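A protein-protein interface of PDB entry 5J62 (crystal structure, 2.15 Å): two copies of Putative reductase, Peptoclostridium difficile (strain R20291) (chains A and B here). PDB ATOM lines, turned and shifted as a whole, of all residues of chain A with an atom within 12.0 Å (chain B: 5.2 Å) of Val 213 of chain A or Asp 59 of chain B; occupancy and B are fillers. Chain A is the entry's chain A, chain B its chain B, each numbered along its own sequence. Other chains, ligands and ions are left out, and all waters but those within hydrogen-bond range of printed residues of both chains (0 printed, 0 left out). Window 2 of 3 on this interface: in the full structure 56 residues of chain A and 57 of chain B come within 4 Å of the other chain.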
ATOM      1  N   LYS A 209      -1.884   7.373  -4.339  1.00  0.00           N
ATOM      2  CA  LYS A 209      -1.731   6.827  -3.017  1.00  0.00           C
ATOM      3  C   LYS A 209      -0.644   5.781  -3.119  1.00  0.00           C
ATOM      4  O   LYS A 209      -0.896   4.555  -3.092  1.00  0.00           O
ATOM      5  CB  LYS A 209      -3.005   6.282  -2.444  1.00  0.00           C
ATOM      6  CG  LYS A 209      -4.148   7.279  -2.417  1.00  0.00           C
ATOM      7  CD  LYS A 209      -5.325   6.811  -1.554  1.00  0.00           C
ATOM      8  CE  LYS A 209      -6.555   7.690  -1.776  1.00  0.00           C
ATOM      9  NZ  LYS A 209      -7.662   7.395  -0.852  1.00  0.00           N
ATOM     10  N   VAL A 210       0.582   6.302  -3.180  1.00  0.00           N
ATOM     11  CA  VAL A 210       1.767   5.533  -3.609  1.00  0.00           C
ATOM     12  C   VAL A 210       2.985   5.741  -2.683  1.00  0.00           C
ATOM     13  O   VAL A 210       3.193   6.841  -2.171  1.00  0.00           O
ATOM     14  CB  VAL A 210       2.109   5.820  -5.079  1.00  0.00           C
ATOM     15  CG1 VAL A 210       2.705   7.203  -5.281  1.00  0.00           C
ATOM     16  CG2 VAL A 210       3.121   4.806  -5.568  1.00  0.00           C
ATOM     17  N   SER A 211       3.750   4.676  -2.453  1.00  0.00           N
ATOM     18  CA  SER A 211       5.106   4.741  -1.855  1.00  0.00           C
ATOM     19  C   SER A 211       6.087   4.182  -2.861  1.00  0.00           C
ATOM     20  O   SER A 211       5.713   3.333  -3.665  1.00  0.00           O
ATOM     21  CB  SER A 211       5.184   3.896  -0.600  1.00  0.00           C
ATOM     22  OG  SER A 211       4.272   4.412   0.381  1.00  0.00           O
ATOM     23  N   ARG A 212       7.342   4.626  -2.817  1.00  0.00           N
ATOM     24  CA  ARG A 212       8.406   4.096  -3.706  1.00  0.00           C
ATOM     25  C   ARG A 212       9.639   3.604  -2.977  1.00  0.00           C
ATOM     26  O   ARG A 212       9.922   4.049  -1.876  1.00  0.00           O
ATOM     27  CB  ARG A 212       8.831   5.135  -4.703  1.00  0.00           C
ATOM     28  CG  ARG A 212       7.749   5.473  -5.679  1.00  0.00           C
ATOM     29  CD  ARG A 212       7.984   6.853  -6.250  1.00  0.00           C
ATOM     30  NE  ARG A 212       7.021   7.171  -7.291  1.00  0.00           N
ATOM     31  CZ  ARG A 212       7.067   6.680  -8.533  1.00  0.00           C
ATOM     32  NH1 ARG A 212       8.027   5.812  -8.929  1.00  0.00           N
ATOM     33  NH2 ARG A 212       6.130   7.050  -9.395  1.00  0.00           N
ATOM     34  N   VAL A 213      10.346   2.663  -3.615  1.00  0.00           N
ATOM     35  CA  VAL A 213      11.666   2.195  -3.177  1.00  0.00           C
ATOM     36  C   VAL A 213      12.585   1.953  -4.409  1.00  0.00           C
ATOM     37  O   VAL A 213      12.608   0.862  -5.026  1.00  0.00           O
ATOM     38  CB  VAL A 213      11.572   0.916  -2.287  1.00  0.00           C
ATOM     39  CG1 VAL A 213      12.910   0.660  -1.602  1.00  0.00           C
ATOM     40  CG2 VAL A 213      10.442   1.007  -1.254  1.00  0.00           C
ATOM     41  N   THR B  55       2.797   0.144  -3.439  1.00  0.00           N
ATOM     42  CA  THR B  55       4.225   0.351  -3.213  1.00  0.00           C
ATOM     43  C   THR B  55       4.961  -0.127  -4.431  1.00  0.00           C
ATOM     44  O   THR B  55       4.828  -1.295  -4.780  1.00  0.00           O
ATOM     45  CB  THR B  55       4.720  -0.402  -1.976  1.00  0.00           C
ATOM     46  OG1 THR B  55       3.966   0.016  -0.841  1.00  0.00           O
ATOM     47  CG2 THR B  55       6.209  -0.081  -1.722  1.00  0.00           C
ATOM     48  N   VAL B  56       5.639   0.783  -5.138  1.00  0.00           N
ATOM     49  CA  VAL B  56       6.467   0.455  -6.325  1.00  0.00           C
ATOM     50  C   VAL B  56       7.839   0.005  -5.838  1.00  0.00           C
ATOM     51  O   VAL B  56       8.489   0.730  -5.069  1.00  0.00           O
ATOM     52  CB  VAL B  56       6.638   1.635  -7.311  1.00  0.00           C
ATOM     53  CG1 VAL B  56       7.455   1.245  -8.552  1.00  0.00           C
ATOM     54  CG2 VAL B  56       5.284   2.182  -7.776  1.00  0.00           C
ATOM     55  N   VAL B  57       8.245  -1.207  -6.233  1.00  0.00           N
ATOM     56  CA  VAL B  57       9.592  -1.714  -5.926  1.00  0.00           C
ATOM     57  C   VAL B  57      10.333  -2.074  -7.204  1.00  0.00           C
ATOM     58  O   VAL B  57       9.859  -2.918  -7.995  1.00  0.00           O
ATOM     59  CB  VAL B  57       9.579  -2.950  -5.007  1.00  0.00           C
ATOM     60  CG1 VAL B  57      11.000  -3.538  -4.822  1.00  0.00           C
ATOM     61  CG2 VAL B  57       8.988  -2.613  -3.634  1.00  0.00           C
ATOM     62  N   GLN B  58      11.493  -1.446  -7.415  1.00  0.00           N
ATOM     63  CA  GLN B  58      12.414  -1.820  -8.506  1.00  0.00           C
ATOM     64  C   GLN B  58      13.811  -2.269  -8.031  1.00  0.00           C
ATOM     65  O   GLN B  58      14.682  -2.571  -8.830  1.00  0.00           O
ATOM     66  CB  GLN B  58      12.523  -0.660  -9.479  1.00  0.00           C
ATOM     67  CG  GLN B  58      11.193  -0.260 -10.044  1.00  0.00           C
ATOM     68  CD  GLN B  58      11.248   0.937 -10.973  1.00  0.00           C
ATOM     69  OE1 GLN B  58      10.770   0.872 -12.086  1.00  0.00           O
ATOM     70  NE2 GLN B  58      11.814   2.029 -10.515  1.00  0.00           N
ATOM     71  N   ASP B  59      13.996  -2.339  -6.718  1.00  0.00           N
ATOM     72  CA  ASP B  59      15.247  -2.744  -6.129  1.00  0.00           C
ATOM     73  C   ASP B  59      15.292  -4.278  -6.144  1.00  0.00           C
ATOM     74  O   ASP B  59      14.611  -4.935  -5.402  1.00  0.00           O
ATOM     75  CB  ASP B  59      15.362  -2.128  -4.715  1.00  0.00           C
ATOM     76  CG  ASP B  59      16.536  -2.706  -3.904  1.00  0.00           C
ATOM     77  OD1 ASP B  59      17.385  -3.426  -4.467  1.00  0.00           O
ATOM     78  OD2 ASP B  59      16.590  -2.460  -2.682  1.00  0.00           O
ATOM     79  N   GLN B  60      16.096  -4.860  -7.007  1.00  0.00           N
ATOM     80  CA  GLN B  60      16.208  -6.334  -7.067  1.00  0.00           C
ATOM     81  C   GLN B  60      16.705  -7.036  -5.778  1.00  0.00           C
ATOM     82  O   GLN B  60      16.357  -8.205  -5.550  1.00  0.00           O
ATOM     83  CB  GLN B  60      17.045  -6.778  -8.286  1.00  0.00           C
ATOM     84  CG  GLN B  60      16.442  -6.402  -9.650  1.00  0.00           C
ATOM     85  CD  GLN B  60      15.026  -6.974  -9.888  1.00  0.00           C
ATOM     86  OE1 GLN B  60      14.148  -6.269 -10.439  1.00  0.00           O
ATOM     87  NE2 GLN B  60      14.787  -8.246  -9.459  1.00  0.00           N
ATOM     88  N   LYS B  61      17.482  -6.325  -4.961  1.00  0.00           N
ATOM     89  CA  LYS B  61      17.989  -6.821  -3.695  1.00  0.00           C
ATOM     90  C   LYS B  61      16.832  -7.045  -2.739  1.00  0.00           C
ATOM     91  O   LYS B  61      16.776  -8.076  -2.061  1.00  0.00           O
ATOM     92  CB  LYS B  61      18.939  -5.798  -3.038  1.00  0.00           C
ATOM     93  CG  LYS B  61      20.435  -6.130  -2.930  1.00  0.00           C
ATOM     94  CD  LYS B  61      21.060  -5.212  -1.853  1.00  0.00           C
ATOM     95  CE  LYS B  61      22.325  -5.742  -1.180  1.00  0.00           C
ATOM     96  NZ  LYS B  61      23.524  -4.985  -1.628  1.00  0.00           N
ATOM     97  N   LEU B  62      15.937  -6.052  -2.659  1.00  0.00           N
ATOM     98  CA  LEU B  62      14.763  -6.164  -1.800  1.00  0.00           C
ATOM     99  C   LEU B  62      13.865  -7.296  -2.304  1.00  0.00           C
ATOM    100  O   LEU B  62      13.420  -8.127  -1.521  1.00  0.00           O
ATOM    101  CB  LEU B  62      13.985  -4.856  -1.743  1.00  0.00           C
ATOM    102  CG  LEU B  62      12.719  -4.840  -0.874  1.00  0.00           C
ATOM    103  CD1 LEU B  62      12.969  -5.279   0.581  1.00  0.00           C
ATOM    104  CD2 LEU B  62      12.163  -3.447  -0.957  1.00  0.00           C
ATOM    105  N   LEU B  63      13.688  -7.383  -3.610  1.00  0.00           N
ATOM    106  CA  LEU B  63      12.780  -8.409  -4.167  1.00  0.00           C
ATOM    107  C   LEU B  63      13.272  -9.839  -3.869  1.00  0.00           C
ATOM    108  O   LEU B  63      12.494 -10.744  -3.520  1.00  0.00           O
ATOM    109  CB  LEU B  63      12.610  -8.159  -5.652  1.00  0.00           C
ATOM    110  CG  LEU B  63      11.829  -6.879  -6.003  1.00  0.00           C
ATOM    111  CD1 LEU B  63      11.780  -6.665  -7.502  1.00  0.00           C
ATOM    112  CD2 LEU B  63      10.402  -6.923  -5.510  1.00  0.00           C
ATOM    113  N   LEU B 178       9.393  -1.980   5.494  1.00  0.00           N
ATOM    114  CA  LEU B 178      10.148  -1.730   4.215  1.00  0.00           C
ATOM    115  C   LEU B 178       9.264  -1.402   3.024  1.00  0.00           C
ATOM    116  O   LEU B 178       9.711  -0.757   2.095  1.00  0.00           O
ATOM    117  CB  LEU B 178      11.033  -2.908   3.802  1.00  0.00           C
ATOM    118  CG  LEU B 178      12.138  -3.270   4.795  1.00  0.00           C
ATOM    119  CD1 LEU B 178      12.750  -4.640   4.480  1.00  0.00           C
ATOM    120  CD2 LEU B 178      13.188  -2.157   4.815  1.00  0.00           C
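The backbone carbonyl oxygen (O) of Ser 211 of chain A sits at hydrogen-bond distance from the backbone NH (N) of Val 56 of chain B (2.9 Å).
The backbone NH of Val 213 of chain A sits at hydrogen-bond distance from the backbone carbonyl oxygen of Val 56 of chain B, 3.0 Å away.
No position is printed for both chains.
Ser 211 of chain A touches Thr 55 of chain B (O to CA, 3.4 Å).
Arg 212 of chain A touches Val 56 of chain B (CA to O, 3.6 Å).
N of Gln 58 of chain B touches O of Val 213 of chain A (3.5 Å).
Val 213 of chain A touches Asp 59 of chain B (O to N, 3.9 Å).
CG2 of Val 213 of chain A touches O of Leu 178 of chain B (3.9 Å).
The side-chain carboxylate (OD1) of Asp 59 of chain B is in hydrogen-bond range of the backbone NH (N) of Lys 61 of chain B (2.9 Å).
Hydrophobic or aromatic side chains of chain A that line the printed part of chain B: Val 213.
Printed residues of chain B that touch a printed residue of chain A: Thr 55, Val 56, Gln 58, Asp 59 and Leu 178.
Among the printed residues, 7 pairs touch across the chains.
Of the printed residues of chain B, Ser 211 of chain A touches Thr 55 (3.4 Å) and Val 56 (2.9 Å).
Of the printed residues of chain B, Arg 212 of chain A touches Val 56.
Val 213 of chain A touches just these residues of chain B: Val 56, Gln 58, Asp 59 and Leu 178.
Of the printed residues of chain A, Thr 55 of chain B touches Ser 211.
Of the printed residues of chain A, Val 56 of chain B touches Ser 211 (2.9 Å), Arg 212 (3.6 Å) and Val 213 (3.0 Å).
Asp 59 of chain B touches one residue of chain A.
No residue of chain A comes within 4 Å of Gln 60 of chain B.
Leu 62 of chain B touches none of the printed residues of chain A.
No residue of chain A comes within 4 Å of Leu 63 of chain B.
Of the printed residues of chain A, Leu 178 of chain B touches Val 213.
The nearest residue of chain B that does not touch Val 213 of chain A is Val 57 of chain B (4.1 Å).
The nearest residue of chain A that does not touch Asp 59 of chain B is Arg 212 of chain A (8.3 Å).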
